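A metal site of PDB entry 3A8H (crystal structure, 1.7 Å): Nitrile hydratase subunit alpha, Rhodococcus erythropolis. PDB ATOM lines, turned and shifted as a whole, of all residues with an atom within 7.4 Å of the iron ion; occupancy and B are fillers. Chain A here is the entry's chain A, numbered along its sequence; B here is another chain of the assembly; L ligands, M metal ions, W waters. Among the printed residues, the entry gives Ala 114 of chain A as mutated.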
ATOM      1  N   GLN A  91      16.227 -14.491  31.660  1.00  0.00           N
ATOM      2  CA  GLN A  91      15.211 -15.444  32.135  1.00  0.00           C
ATOM      3  C   GLN A  91      15.495 -15.897  33.576  1.00  0.00           C
ATOM      4  O   GLN A  91      15.203 -17.017  33.976  1.00  0.00           O
ATOM      5  CB  GLN A  91      15.058 -16.629  31.159  1.00  0.00           C
ATOM      6  CG  GLN A  91      14.531 -16.202  29.783  1.00  0.00           C
ATOM      7  CD  GLN A  91      13.213 -15.512  29.921  1.00  0.00           C
ATOM      8  OE1 GLN A  91      12.258 -16.106  30.428  1.00  0.00           O
ATOM      9  NE2 GLN A  91      13.142 -14.255  29.486  1.00  0.00           N
ATOM     10  N   VAL A 109       6.341 -25.599  36.322  1.00  0.00           N
ATOM     11  CA  VAL A 109       6.078 -25.790  34.883  1.00  0.00           C
ATOM     12  C   VAL A 109       5.896 -24.414  34.226  1.00  0.00           C
ATOM     13  O   VAL A 109       5.689 -23.408  34.923  1.00  0.00           O
ATOM     14  CB  VAL A 109       4.795 -26.630  34.677  1.00  0.00           C
ATOM     15  CG1 VAL A 109       3.554 -25.883  35.213  1.00  0.00           C
ATOM     16  CG2 VAL A 109       4.604 -26.980  33.204  1.00  0.00           C
ATOM     17  N   CYS A 110       5.959 -24.381  32.889  1.00  0.00           N
ATOM     18  CA  CYS A 110       5.421 -23.256  32.136  1.00  0.00           C
ATOM     19  C   CYS A 110       4.366 -23.825  31.186  1.00  0.00           C
ATOM     20  O   CYS A 110       4.709 -24.302  30.079  1.00  0.00           O
ATOM     21  CB  CYS A 110       6.502 -22.526  31.356  1.00  0.00           C
ATOM     22  SG  CYS A 110       5.857 -21.181  30.327  1.00  0.00           S
ATOM     23  N   SER A 111       3.104 -23.825  31.600  1.00  0.00           N
ATOM     24  CA  SER A 111       2.075 -24.482  30.790  1.00  0.00           C
ATOM     25  C   SER A 111       1.927 -23.794  29.425  1.00  0.00           C
ATOM     26  O   SER A 111       1.516 -24.429  28.461  1.00  0.00           O
ATOM     27  CB  SER A 111       0.720 -24.531  31.493  1.00  0.00           C
ATOM     28  OG  SER A 111       0.154 -23.239  31.643  1.00  0.00           O
ATOM     29  N   LEU A 112       2.255 -22.507  29.370  1.00  0.00           N
ATOM     30  CA  LEU A 112       2.000 -21.699  28.158  1.00  0.00           C
ATOM     31  C   LEU A 112       3.155 -21.752  27.156  1.00  0.00           C
ATOM     32  O   LEU A 112       2.968 -21.383  26.002  1.00  0.00           O
ATOM     33  CB  LEU A 112       1.695 -20.236  28.545  1.00  0.00           C
ATOM     34  CG  LEU A 112       0.402 -20.030  29.340  1.00  0.00           C
ATOM     35  CD1 LEU A 112       0.352 -18.581  29.831  1.00  0.00           C
ATOM     36  CD2 LEU A 112      -0.834 -20.354  28.499  1.00  0.00           C
ATOM     37  N   CSD A 113       4.318 -22.217  27.585  1.00  0.00           N
ATOM     38  CA  CSD A 113       5.513 -22.293  26.710  1.00  0.00           C
ATOM     39  CB  CSD A 113       5.997 -20.926  26.188  1.00  0.00           C
ATOM     40  SG  CSD A 113       6.179 -19.720  27.504  1.00  0.00           S
ATOM     41  C   CSD A 113       6.635 -23.113  27.340  1.00  0.00           C
ATOM     42  O   CSD A 113       6.654 -24.352  27.161  1.00  0.00           O
ATOM     43  OD1 CSD A 113       6.805 -18.551  26.721  1.00  0.00           O
ATOM     44  OD2 CSD A 113       4.771 -19.351  27.994  1.00  0.00           O
ATOM     45  N   ALA A 114       7.586 -22.481  28.024  1.00  0.00           N
ATOM     46  CA  ALA A 114       8.746 -23.239  28.578  1.00  0.00           C
ATOM     47  C   ALA A 114       9.511 -22.494  29.648  1.00  0.00           C
ATOM     48  O   ALA A 114      10.600 -22.938  30.078  1.00  0.00           O
ATOM     49  CB  ALA A 114       9.698 -23.665  27.432  1.00  0.00           C
ATOM     50  N   CSO A 115       8.932 -21.376  30.069  1.00  0.00           N
ATOM     51  CA  CSO A 115       9.583 -20.485  31.025  1.00  0.00           C
ATOM     52  CB  CSO A 115       8.616 -19.380  31.491  1.00  0.00           C
ATOM     53  SG  CSO A 115       7.798 -18.667  30.034  1.00  0.00           S
ATOM     54  C   CSO A 115      10.252 -21.226  32.192  1.00  0.00           C
ATOM     55  O   CSO A 115       9.644 -22.062  32.865  1.00  0.00           O
ATOM     56  OD  CSO A 115       9.011 -17.734  29.210  1.00  0.00           O
ATOM     57  N   THR A 116      11.523 -20.888  32.390  1.00  0.00           N
ATOM     58  CA  THR A 116      12.457 -21.590  33.266  1.00  0.00           C
ATOM     59  C   THR A 116      13.486 -20.580  33.748  1.00  0.00           C
ATOM     60  O   THR A 116      13.882 -19.701  32.986  1.00  0.00           O
ATOM     61  CB  THR A 116      13.172 -22.679  32.434  1.00  0.00           C
ATOM     62  OG1 THR A 116      12.231 -23.698  32.093  1.00  0.00           O
ATOM     63  CG2 THR A 116      14.364 -23.302  33.169  1.00  0.00           C
ATOM     64  N   PRO A 124      15.611 -25.325  29.595  1.00  0.00           N
ATOM     65  CA  PRO A 124      14.738 -26.466  29.900  1.00  0.00           C
ATOM     66  C   PRO A 124      15.007 -27.657  28.999  1.00  0.00           C
ATOM     67  O   PRO A 124      15.393 -27.489  27.840  1.00  0.00           O
ATOM     68  CB  PRO A 124      13.326 -25.934  29.631  1.00  0.00           C
ATOM     69  CG  PRO A 124      13.503 -24.711  28.740  1.00  0.00           C
ATOM     70  CD  PRO A 124      14.853 -24.135  29.164  1.00  0.00           C
ATOM     71  N   TYR A 128      10.378 -31.116  29.562  1.00  0.00           N
ATOM     72  CA  TYR A 128       9.708 -30.037  30.322  1.00  0.00           C
ATOM     73  C   TYR A 128       8.897 -29.175  29.351  1.00  0.00           C
ATOM     74  O   TYR A 128       7.865 -28.590  29.710  1.00  0.00           O
ATOM     75  CB  TYR A 128      10.768 -29.224  31.067  1.00  0.00           C
ATOM     76  CG  TYR A 128      10.297 -27.997  31.823  1.00  0.00           C
ATOM     77  CD1 TYR A 128      10.177 -26.759  31.168  1.00  0.00           C
ATOM     78  CD2 TYR A 128      10.018 -28.074  33.174  1.00  0.00           C
ATOM     79  CE1 TYR A 128       9.776 -25.611  31.871  1.00  0.00           C
ATOM     80  CE2 TYR A 128       9.616 -26.939  33.884  1.00  0.00           C
ATOM     81  CZ  TYR A 128       9.512 -25.715  33.236  1.00  0.00           C
ATOM     82  OH  TYR A 128       9.156 -24.590  33.945  1.00  0.00           O
ATOM     83  N   ARG A 134       3.269 -29.997  29.968  1.00  0.00           N
ATOM     84  CA  ARG A 134       2.539 -28.724  30.006  1.00  0.00           C
ATOM     85  C   ARG A 134       1.045 -28.906  30.239  1.00  0.00           C
ATOM     86  O   ARG A 134       0.416 -28.101  30.941  1.00  0.00           O
ATOM     87  CB  ARG A 134       2.789 -27.970  28.682  1.00  0.00           C
ATOM     88  CG  ARG A 134       4.201 -27.432  28.595  1.00  0.00           C
ATOM     89  CD  ARG A 134       4.511 -26.739  27.255  1.00  0.00           C
ATOM     90  NE  ARG A 134       3.427 -25.815  26.910  1.00  0.00           N
ATOM     91  CZ  ARG A 134       3.185 -25.375  25.688  1.00  0.00           C
ATOM     92  NH1 ARG A 134       3.944 -25.778  24.671  1.00  0.00           N
ATOM     93  NH2 ARG A 134       2.142 -24.576  25.459  1.00  0.00           N
ATOM     94  N   THR A 163       4.652 -20.946  35.587  1.00  0.00           N
ATOM     95  CA  THR A 163       5.525 -19.806  35.324  1.00  0.00           C
ATOM     96  C   THR A 163       4.933 -18.937  34.210  1.00  0.00           C
ATOM     97  O   THR A 163       5.338 -19.040  33.043  1.00  0.00           O
ATOM     98  CB  THR A 163       6.976 -20.264  34.973  1.00  0.00           C
ATOM     99  OG1 THR A 163       7.465 -21.178  35.967  1.00  0.00           O
ATOM    100  CG2 THR A 163       7.934 -19.082  34.887  1.00  0.00           C
ATOM    101  N   THR A 164       3.992 -18.079  34.576  1.00  0.00           N
ATOM    102  CA  THR A 164       3.151 -17.347  33.630  1.00  0.00           C
ATOM    103  C   THR A 164       3.562 -15.892  33.416  1.00  0.00           C
ATOM    104  O   THR A 164       3.060 -15.214  32.507  1.00  0.00           O
ATOM    105  CB  THR A 164       1.689 -17.407  34.079  1.00  0.00           C
ATOM    106  OG1 THR A 164       1.612 -17.084  35.476  1.00  0.00           O
ATOM    107  CG2 THR A 164       1.109 -18.808  33.885  1.00  0.00           C
ATOM    108  N   ARG A 168      10.812 -16.287  38.174  1.00  0.00           N
ATOM    109  CA  ARG A 168      11.459 -17.523  37.749  1.00  0.00           C
ATOM    110  C   ARG A 168      11.775 -18.291  39.011  1.00  0.00           C
ATOM    111  O   ARG A 168      12.348 -17.747  39.970  1.00  0.00           O
ATOM    112  CB  ARG A 168      12.706 -17.218  36.927  1.00  0.00           C
ATOM    113  CG  ARG A 168      12.381 -16.505  35.607  1.00  0.00           C
ATOM    114  CD  ARG A 168      11.816 -17.490  34.592  1.00  0.00           C
ATOM    115  NE  ARG A 168      11.403 -16.811  33.350  1.00  0.00           N
ATOM    116  CZ  ARG A 168      10.234 -16.193  33.173  1.00  0.00           C
ATOM    117  NH1 ARG A 168       9.314 -16.173  34.137  1.00  0.00           N
ATOM    118  NH2 ARG A 168       9.962 -15.591  32.026  1.00  0.00           N
ATOM    119  N   ARG B  56       6.640 -14.513  22.289  1.00  0.00           N
ATOM    120  CA  ARG B  56       5.658 -15.482  22.799  1.00  0.00           C
ATOM    121  C   ARG B  56       4.392 -15.412  21.955  1.00  0.00           C
ATOM    122  O   ARG B  56       3.826 -16.448  21.561  1.00  0.00           O
ATOM    123  CB  ARG B  56       5.301 -15.207  24.260  1.00  0.00           C
ATOM    124  CG  ARG B  56       6.443 -15.437  25.227  1.00  0.00           C
ATOM    125  CD  ARG B  56       5.906 -15.465  26.646  1.00  0.00           C
ATOM    126  NE  ARG B  56       7.042 -15.689  27.549  1.00  0.00           N
ATOM    127  CZ  ARG B  56       7.763 -14.715  28.082  1.00  0.00           C
ATOM    128  NH1 ARG B  56       7.463 -13.447  27.840  1.00  0.00           N
ATOM    129  NH2 ARG B  56       8.801 -15.012  28.870  1.00  0.00           N
ATOM    130  N   TYR B  72       9.639 -27.735  19.739  1.00  0.00           N
ATOM    131  CA  TYR B  72       9.876 -26.456  20.405  1.00  0.00           C
ATOM    132  C   TYR B  72      10.840 -25.467  19.691  1.00  0.00           C
ATOM    133  O   TYR B  72      10.431 -24.365  19.339  1.00  0.00           O
ATOM    134  CB  TYR B  72      10.406 -26.745  21.814  1.00  0.00           C
ATOM    135  CG  TYR B  72      10.683 -25.488  22.578  1.00  0.00           C
ATOM    136  CD1 TYR B  72       9.673 -24.878  23.313  1.00  0.00           C
ATOM    137  CD2 TYR B  72      11.960 -24.907  22.585  1.00  0.00           C
ATOM    138  CE1 TYR B  72       9.908 -23.726  24.011  1.00  0.00           C
ATOM    139  CE2 TYR B  72      12.209 -23.728  23.291  1.00  0.00           C
ATOM    140  CZ  TYR B  72      11.179 -23.153  24.004  1.00  0.00           C
ATOM    141  OH  TYR B  72      11.381 -21.988  24.710  1.00  0.00           O
ATOM    142  N   TYR B  76      10.327 -21.425  17.520  1.00  0.00           N
ATOM    143  CA  TYR B  76      11.006 -20.127  17.695  1.00  0.00           C
ATOM    144  C   TYR B  76      11.749 -19.654  16.451  1.00  0.00           C
ATOM    145  O   TYR B  76      11.815 -18.460  16.197  1.00  0.00           O
ATOM    146  CB  TYR B  76      11.869 -20.118  18.975  1.00  0.00           C
ATOM    147  CG  TYR B  76      10.913 -20.265  20.160  1.00  0.00           C
ATOM    148  CD1 TYR B  76      10.330 -19.149  20.758  1.00  0.00           C
ATOM    149  CD2 TYR B  76      10.451 -21.531  20.543  1.00  0.00           C
ATOM    150  CE1 TYR B  76       9.384 -19.289  21.809  1.00  0.00           C
ATOM    151  CE2 TYR B  76       9.497 -21.689  21.544  1.00  0.00           C
ATOM    152  CZ  TYR B  76       8.966 -20.577  22.170  1.00  0.00           C
ATOM    153  OH  TYR B  76       8.051 -20.779  23.169  1.00  0.00           O
ATOM    154  N   ARG B 141      -1.257 -13.322  29.481  1.00  0.00           N
ATOM    155  CA  ARG B 141      -0.529 -14.281  30.309  1.00  0.00           C
ATOM    156  C   ARG B 141      -1.418 -14.852  31.417  1.00  0.00           C
ATOM    157  O   ARG B 141      -1.005 -15.016  32.554  1.00  0.00           O
ATOM    158  CB  ARG B 141       0.768 -13.653  30.855  1.00  0.00           C
ATOM    159  CG  ARG B 141       1.769 -13.350  29.752  1.00  0.00           C
ATOM    160  CD  ARG B 141       2.086 -14.621  28.932  1.00  0.00           C
ATOM    161  NE  ARG B 141       2.907 -15.563  29.710  1.00  0.00           N
ATOM    162  CZ  ARG B 141       3.386 -16.714  29.246  1.00  0.00           C
ATOM    163  NH1 ARG B 141       3.079 -17.106  28.027  1.00  0.00           N
ATOM    164  NH2 ARG B 141       4.172 -17.462  30.023  1.00  0.00           N
HETATM  165  C1  LIG L   1      11.491 -16.940  23.971  1.00  0.00           C
HETATM  166  C2  LIG L   1       9.919 -16.755  25.907  1.00  0.00           C
HETATM  167  C3  LIG L   1      12.372 -16.495  26.255  1.00  0.00           C
HETATM  168  N1  LIG L   1      10.774 -19.470  24.742  1.00  0.00           N
HETATM  169  O1  LIG L   1      11.965 -19.211  26.622  1.00  0.00           O
HETATM  170  C4  LIG L   1      11.388 -18.715  25.665  1.00  0.00           C
HETATM  171  C5  LIG L   1      11.293 -17.214  25.457  1.00  0.00           C
HETATM  172 FE    FE M   1       7.572 -20.570  28.867  1.00  0.00          FE
HETATM  173  O   HOH W   1       9.116 -20.043  27.561  1.00  0.00           O
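A nitrogen (N1) of the ligand sits close to the side-chain hydroxyl (OH) of Tyr 76 of chain B, 3.4 Å away.
The side-chain hydroxyl (OH) of Tyr 72 of chain B is in hydrogen-bond range of a nitrogen (N1) of the ligand.
The guanidinium group (NH2) of Arg 56 of chain B lies within hydrogen-bond range of OD of CSO 115 (2.8 Å).
The side-chain hydroxyl (OH) of Tyr 128 lies within hydrogen-bond range of O of CSO 115, at 2.8 Å.
The backbone carbonyl oxygen (O) of Ala 114 lies within hydrogen-bond range of the side-chain hydroxyl (OG1) of Thr 116, 2.7 Å away.
OD2 of CSD 113 lies within salt-bridge range of the guanidinium group of Arg 141 of chain B (2.8 Å).
OD1 of CSD 113 is in salt-bridge range of the guanidinium group (NE) of Arg 56 of chain B (3.0 Å).
SG of Cys 110 lies close to O of Thr 163 (3.5 Å).
The backbone NH of Cys 110 is in hydrogen-bond range of the side-chain hydroxyl of Tyr 128, 3.4 Å away.
Four residues have an atom within 4 Å of the iron ion: Cys 110, CSD 113, Ala 114 and CSO 115.
The iron ion is bound by N of CSO 115 (2.0 Å), N of Ala 114 (2.1 Å), water W1 (2.1 Å), SG of CSD 113 (2.1 Å), SG of CSO 115 (2.2 Å) and SG of Cys 110 (2.3 Å).
Water W1 lies within hydrogen-bond range of OD of CSO 115, OD1 of CSD 113 and an oxygen (O1) of the ligand.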
